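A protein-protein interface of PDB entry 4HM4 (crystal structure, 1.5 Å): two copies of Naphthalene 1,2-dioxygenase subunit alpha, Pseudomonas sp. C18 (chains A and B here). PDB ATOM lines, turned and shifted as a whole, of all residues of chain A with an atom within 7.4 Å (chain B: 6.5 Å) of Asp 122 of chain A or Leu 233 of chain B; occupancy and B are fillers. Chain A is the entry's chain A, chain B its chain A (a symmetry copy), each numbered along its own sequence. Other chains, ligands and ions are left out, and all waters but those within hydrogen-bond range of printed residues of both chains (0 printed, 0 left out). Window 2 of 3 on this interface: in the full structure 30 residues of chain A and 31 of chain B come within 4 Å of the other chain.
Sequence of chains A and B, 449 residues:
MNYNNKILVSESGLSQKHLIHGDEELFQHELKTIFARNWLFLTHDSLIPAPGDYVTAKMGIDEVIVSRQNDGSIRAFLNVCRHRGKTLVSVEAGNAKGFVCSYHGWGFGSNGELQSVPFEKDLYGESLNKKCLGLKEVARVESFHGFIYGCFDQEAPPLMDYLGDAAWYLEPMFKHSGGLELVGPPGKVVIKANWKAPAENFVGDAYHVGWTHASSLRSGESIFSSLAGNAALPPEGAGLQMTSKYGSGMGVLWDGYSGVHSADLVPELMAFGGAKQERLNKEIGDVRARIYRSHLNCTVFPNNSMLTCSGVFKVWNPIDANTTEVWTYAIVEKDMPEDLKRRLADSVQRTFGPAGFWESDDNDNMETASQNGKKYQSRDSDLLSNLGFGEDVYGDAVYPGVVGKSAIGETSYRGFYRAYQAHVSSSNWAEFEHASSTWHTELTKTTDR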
ATOM      1  N   PRO A 118       9.892 -33.706 -22.275  1.00  0.00           N
ATOM      2  CA  PRO A 118      10.031 -32.258 -22.047  1.00  0.00           C
ATOM      3  C   PRO A 118       8.887 -31.456 -22.648  1.00  0.00           C
ATOM      4  O   PRO A 118       8.560 -31.658 -23.819  1.00  0.00           O
ATOM      5  CB  PRO A 118      11.341 -31.917 -22.765  1.00  0.00           C
ATOM      6  CG  PRO A 118      12.132 -33.184 -22.689  1.00  0.00           C
ATOM      7  CD  PRO A 118      11.111 -34.283 -22.871  1.00  0.00           C
ATOM      8  N   PHE A 119       8.285 -30.582 -21.841  1.00  0.00           N
ATOM      9  CA  PHE A 119       7.202 -29.703 -22.280  1.00  0.00           C
ATOM     10  C   PHE A 119       6.012 -30.480 -22.824  1.00  0.00           C
ATOM     11  O   PHE A 119       5.366 -30.042 -23.772  1.00  0.00           O
ATOM     12  CB  PHE A 119       7.700 -28.721 -23.344  1.00  0.00           C
ATOM     13  CG  PHE A 119       8.903 -27.928 -22.924  1.00  0.00           C
ATOM     14  CD1 PHE A 119       8.846 -27.078 -21.831  1.00  0.00           C
ATOM     15  CD2 PHE A 119      10.084 -28.020 -23.640  1.00  0.00           C
ATOM     16  CE1 PHE A 119       9.963 -26.338 -21.446  1.00  0.00           C
ATOM     17  CE2 PHE A 119      11.200 -27.284 -23.273  1.00  0.00           C
ATOM     18  CZ  PHE A 119      11.140 -26.446 -22.172  1.00  0.00           C
ATOM     19  N   GLU A 120       5.721 -31.622 -22.214  1.00  0.00           N
ATOM     20  CA  GLU A 120       4.690 -32.510 -22.733  1.00  0.00           C
ATOM     21  C   GLU A 120       3.347 -31.803 -22.873  1.00  0.00           C
ATOM     22  O   GLU A 120       2.687 -31.919 -23.904  1.00  0.00           O
ATOM     23  CB  GLU A 120       4.549 -33.763 -21.869  1.00  0.00           C
ATOM     24  CG  GLU A 120       3.524 -34.745 -22.409  1.00  0.00           C
ATOM     25  CD  GLU A 120       3.319 -35.957 -21.516  1.00  0.00           C
ATOM     26  OE1 GLU A 120       3.939 -36.037 -20.431  1.00  0.00           O
ATOM     27  OE2 GLU A 120       2.532 -36.837 -21.911  1.00  0.00           O
ATOM     28  N   LYS A 121       2.959 -31.044 -21.854  1.00  0.00           N
ATOM     29  CA  LYS A 121       1.668 -30.361 -21.864  1.00  0.00           C
ATOM     30  C   LYS A 121       1.535 -29.391 -23.046  1.00  0.00           C
ATOM     31  O   LYS A 121       0.533 -29.401 -23.764  1.00  0.00           O
ATOM     32  CB  LYS A 121       1.464 -29.618 -20.539  1.00  0.00           C
ATOM     33  CG  LYS A 121       0.143 -28.867 -20.433  1.00  0.00           C
ATOM     34  CD  LYS A 121      -1.047 -29.811 -20.427  1.00  0.00           C
ATOM     35  CE  LYS A 121      -2.015 -29.457 -19.305  1.00  0.00           C
ATOM     36  NZ  LYS A 121      -1.364 -29.543 -17.957  1.00  0.00           N
ATOM     37  N   ASP A 122       2.560 -28.572 -23.258  1.00  0.00           N
ATOM     38  CA  ASP A 122       2.513 -27.551 -24.298  1.00  0.00           C
ATOM     39  C   ASP A 122       2.639 -28.135 -25.701  1.00  0.00           C
ATOM     40  O   ASP A 122       2.087 -27.579 -26.651  1.00  0.00           O
ATOM     41  CB  ASP A 122       3.611 -26.510 -24.086  1.00  0.00           C
ATOM     42  CG  ASP A 122       3.282 -25.520 -22.981  1.00  0.00           C
ATOM     43  OD1 ASP A 122       2.372 -24.687 -23.179  1.00  0.00           O
ATOM     44  OD2 ASP A 122       3.948 -25.560 -21.926  1.00  0.00           O
ATOM     45  N   LEU A 123       3.363 -29.249 -25.826  1.00  0.00           N
ATOM     46  CA  LEU A 123       3.676 -29.837 -27.131  1.00  0.00           C
ATOM     47  C   LEU A 123       2.710 -30.941 -27.543  1.00  0.00           C
ATOM     48  O   LEU A 123       2.107 -30.880 -28.616  1.00  0.00           O
ATOM     49  CB  LEU A 123       5.111 -30.381 -27.137  1.00  0.00           C
ATOM     50  CG  LEU A 123       6.181 -29.304 -26.941  1.00  0.00           C
ATOM     51  CD1 LEU A 123       7.576 -29.911 -26.877  1.00  0.00           C
ATOM     52  CD2 LEU A 123       6.100 -28.277 -28.056  1.00  0.00           C
ATOM     53  N   TYR A 124       2.577 -31.955 -26.696  1.00  0.00           N
ATOM     54  CA  TYR A 124       1.736 -33.104 -27.022  1.00  0.00           C
ATOM     55  C   TYR A 124       0.330 -32.981 -26.465  1.00  0.00           C
ATOM     56  O   TYR A 124      -0.569 -33.696 -26.894  1.00  0.00           O
ATOM     57  CB  TYR A 124       2.361 -34.396 -26.499  1.00  0.00           C
ATOM     58  CG  TYR A 124       3.644 -34.782 -27.201  1.00  0.00           C
ATOM     59  CD1 TYR A 124       3.618 -35.509 -28.385  1.00  0.00           C
ATOM     60  CD2 TYR A 124       4.878 -34.419 -26.679  1.00  0.00           C
ATOM     61  CE1 TYR A 124       4.786 -35.869 -29.029  1.00  0.00           C
ATOM     62  CE2 TYR A 124       6.050 -34.767 -27.316  1.00  0.00           C
ATOM     63  CZ  TYR A 124       5.996 -35.496 -28.488  1.00  0.00           C
ATOM     64  OH  TYR A 124       7.156 -35.848 -29.122  1.00  0.00           O
ATOM     65  N   GLY A 125       0.146 -32.078 -25.506  1.00  0.00           N
ATOM     66  CA  GLY A 125      -1.113 -31.993 -24.792  1.00  0.00           C
ATOM     67  C   GLY A 125      -1.380 -33.309 -24.088  1.00  0.00           C
ATOM     68  O   GLY A 125      -0.535 -33.803 -23.339  1.00  0.00           O
ATOM     69  N   SER B 226      18.264 -18.918 -24.462  1.00  0.00           N
ATOM     70  CA  SER B 226      17.350 -19.145 -23.346  1.00  0.00           C
ATOM     71  C   SER B 226      16.829 -20.572 -23.355  1.00  0.00           C
ATOM     72  O   SER B 226      16.165 -21.014 -22.414  1.00  0.00           O
ATOM     73  CB  SER B 226      16.169 -18.199 -23.444  1.00  0.00           C
ATOM     74  OG  SER B 226      15.457 -18.420 -24.654  1.00  0.00           O
ATOM     75  N   LEU B 227      17.115 -21.279 -24.441  1.00  0.00           N
ATOM     76  CA  LEU B 227      16.657 -22.642 -24.616  1.00  0.00           C
ATOM     77  C   LEU B 227      17.531 -23.637 -23.855  1.00  0.00           C
ATOM     78  O   LEU B 227      17.131 -24.769 -23.660  1.00  0.00           O
ATOM     79  CB  LEU B 227      16.641 -22.996 -26.106  1.00  0.00           C
ATOM     80  CG  LEU B 227      15.657 -22.231 -26.988  1.00  0.00           C
ATOM     81  CD1 LEU B 227      15.783 -22.650 -28.446  1.00  0.00           C
ATOM     82  CD2 LEU B 227      14.262 -22.478 -26.498  1.00  0.00           C
ATOM     83  N   ASN B 230      16.680 -26.970 -21.805  1.00  0.00           N
ATOM     84  CA  ASN B 230      15.219 -26.871 -21.728  1.00  0.00           C
ATOM     85  C   ASN B 230      14.746 -25.997 -20.572  1.00  0.00           C
ATOM     86  O   ASN B 230      13.733 -26.272 -19.931  1.00  0.00           O
ATOM     87  CB  ASN B 230      14.571 -28.258 -21.672  1.00  0.00           C
ATOM     88  CG  ASN B 230      14.565 -28.944 -23.020  1.00  0.00           C
ATOM     89  OD1 ASN B 230      14.707 -28.295 -24.059  1.00  0.00           O
ATOM     90  ND2 ASN B 230      14.393 -30.258 -23.012  1.00  0.00           N
ATOM     91  N   ALA B 231      15.505 -24.938 -20.317  1.00  0.00           N
ATOM     92  CA  ALA B 231      15.205 -24.018 -19.232  1.00  0.00           C
ATOM     93  C   ALA B 231      13.962 -23.203 -19.542  1.00  0.00           C
ATOM     94  O   ALA B 231      13.266 -22.753 -18.633  1.00  0.00           O
ATOM     95  CB  ALA B 231      16.381 -23.102 -18.987  1.00  0.00           C
ATOM     96  N   ALA B 232      13.692 -23.002 -20.828  1.00  0.00           N
ATOM     97  CA  ALA B 232      12.553 -22.188 -21.231  1.00  0.00           C
ATOM     98  C   ALA B 232      11.980 -22.614 -22.575  1.00  0.00           C
ATOM     99  O   ALA B 232      12.710 -22.753 -23.560  1.00  0.00           O
ATOM    100  CB  ALA B 232      12.946 -20.714 -21.266  1.00  0.00           C
ATOM    101  N   LEU B 233      10.668 -22.818 -22.612  1.00  0.00           N
ATOM    102  CA  LEU B 233       9.987 -23.083 -23.869  1.00  0.00           C
ATOM    103  C   LEU B 233       9.731 -21.754 -24.560  1.00  0.00           C
ATOM    104  O   LEU B 233       9.273 -20.803 -23.922  1.00  0.00           O
ATOM    105  CB  LEU B 233       8.657 -23.800 -23.626  1.00  0.00           C
ATOM    106  CG  LEU B 233       7.920 -24.240 -24.896  1.00  0.00           C
ATOM    107  CD1 LEU B 233       8.644 -25.397 -25.564  1.00  0.00           C
ATOM    108  CD2 LEU B 233       6.482 -24.614 -24.595  1.00  0.00           C
ATOM    109  N   PRO B 234      10.047 -21.677 -25.861  1.00  0.00           N
ATOM    110  CA  PRO B 234       9.696 -20.494 -26.650  1.00  0.00           C
ATOM    111  C   PRO B 234       8.222 -20.154 -26.473  1.00  0.00           C
ATOM    112  O   PRO B 234       7.394 -21.058 -26.358  1.00  0.00           O
ATOM    113  CB  PRO B 234       9.967 -20.947 -28.086  1.00  0.00           C
ATOM    114  CG  PRO B 234      11.057 -21.949 -27.949  1.00  0.00           C
ATOM    115  CD  PRO B 234      10.787 -22.672 -26.653  1.00  0.00           C
ATOM    116  N   PRO B 235       7.898 -18.858 -26.429  1.00  0.00           N
ATOM    117  CA  PRO B 235       6.515 -18.410 -26.261  1.00  0.00           C
ATOM    118  C   PRO B 235       5.646 -18.875 -27.418  1.00  0.00           C
ATOM    119  O   PRO B 235       6.184 -19.239 -28.464  1.00  0.00           O
ATOM    120  CB  PRO B 235       6.643 -16.887 -26.310  1.00  0.00           C
ATOM    121  CG  PRO B 235       7.921 -16.616 -27.004  1.00  0.00           C
ATOM    122  CD  PRO B 235       8.828 -17.730 -26.607  1.00  0.00           C
ATOM    123  N   GLU B 236       4.328 -18.864 -27.247  1.00  0.00           N
ATOM    124  CA  GLU B 236       3.448 -19.143 -28.374  1.00  0.00           C
ATOM    125  C   GLU B 236       3.702 -18.058 -29.413  1.00  0.00           C
ATOM    126  O   GLU B 236       4.008 -16.915 -29.063  1.00  0.00           O
ATOM    127  CB  GLU B 236       1.974 -19.179 -27.941  1.00  0.00           C
ATOM    128  CG  GLU B 236       1.086 -18.073 -28.523  1.00  0.00           C
ATOM    129  CD  GLU B 236       0.641 -18.354 -29.949  1.00  0.00           C
ATOM    130  OE1 GLU B 236       0.965 -19.446 -30.465  1.00  0.00           O
ATOM    131  OE2 GLU B 236      -0.021 -17.482 -30.555  1.00  0.00           O
ATOM    132  N   ILE B 408       7.780 -25.559 -32.398  1.00  0.00           N
ATOM    133  CA  ILE B 408       8.329 -26.892 -32.161  1.00  0.00           C
ATOM    134  C   ILE B 408       7.318 -27.987 -32.490  1.00  0.00           C
ATOM    135  O   ILE B 408       6.246 -28.054 -31.887  1.00  0.00           O
ATOM    136  CB  ILE B 408       8.747 -27.061 -30.695  1.00  0.00           C
ATOM    137  CG1 ILE B 408       9.825 -26.041 -30.333  1.00  0.00           C
ATOM    138  CG2 ILE B 408       9.239 -28.482 -30.430  1.00  0.00           C
ATOM    139  CD1 ILE B 408      10.239 -26.095 -28.885  1.00  0.00           C
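No position is printed for both chains. Of the 6 pairs that touch across the chains among the printed residues, none has its exchanged pair printed and touching as well.
Asp 122 of chain A touches just one residue of chain B: Leu 233. Leu 233 of chain B touches just these residues of chain A: Phe 119 (3.6 Å) and Asp 122 (3.5 Å). Of the printed residues of chain A, Ala 232 of chain B touches Phe 119. Of the printed residues of chain B, Leu 123 of chain A touches Ile 408. Of the printed residues of chain B, Phe 119 of chain A touches Asn 230, Ala 232 and Leu 233. Printed residues of chain A within 4 Å of Ile 408 of chain B: Leu 123. Pro 235 of chain B touches none of the printed residues of chain A. Leu 227 of chain B touches none of the printed residues of chain A. The nearest printed residue of chain B that does not touch Asp 122 of chain A is Ile 408 of chain B (6.7 Å). The nearest residue of chain A that does not touch Leu 233 of chain B is Leu 123 of chain A (4.6 Å).
Of the 10 printed residues of chain B, 4 touch a printed residue of chain A. Hydrophobic or aromatic side chains of chain B within 4 Å of the printed part of chain A: Leu 233 and Ile 408. Of the 8 printed residues of chain A, 4 touch a printed residue of chain B. Printed residues of chain A that touch a printed residue of chain B: Pro 118, Phe 119, Asp 122 and Leu 123. Among the printed residues, 6 pairs touch across the chains. Among the printed residues, no Asp or Glu carboxylate lies within 4 Å of a Lys or Arg side-chain nitrogen of the other chain.
Asn 230 of chain B touches Pro 118 of chain A. Asn 230 of chain B touches Phe 119 of chain A. C of Ala 232 of chain B touches CZ of Phe 119 of chain A (3.9 Å). Phe 119 of chain A touches Leu 233 of chain B (CD2 to CD1, 3.6 Å). Asp 122 of chain A touches Leu 233 of chain B. Ile 408 of chain B touches Leu 123 of chain A.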
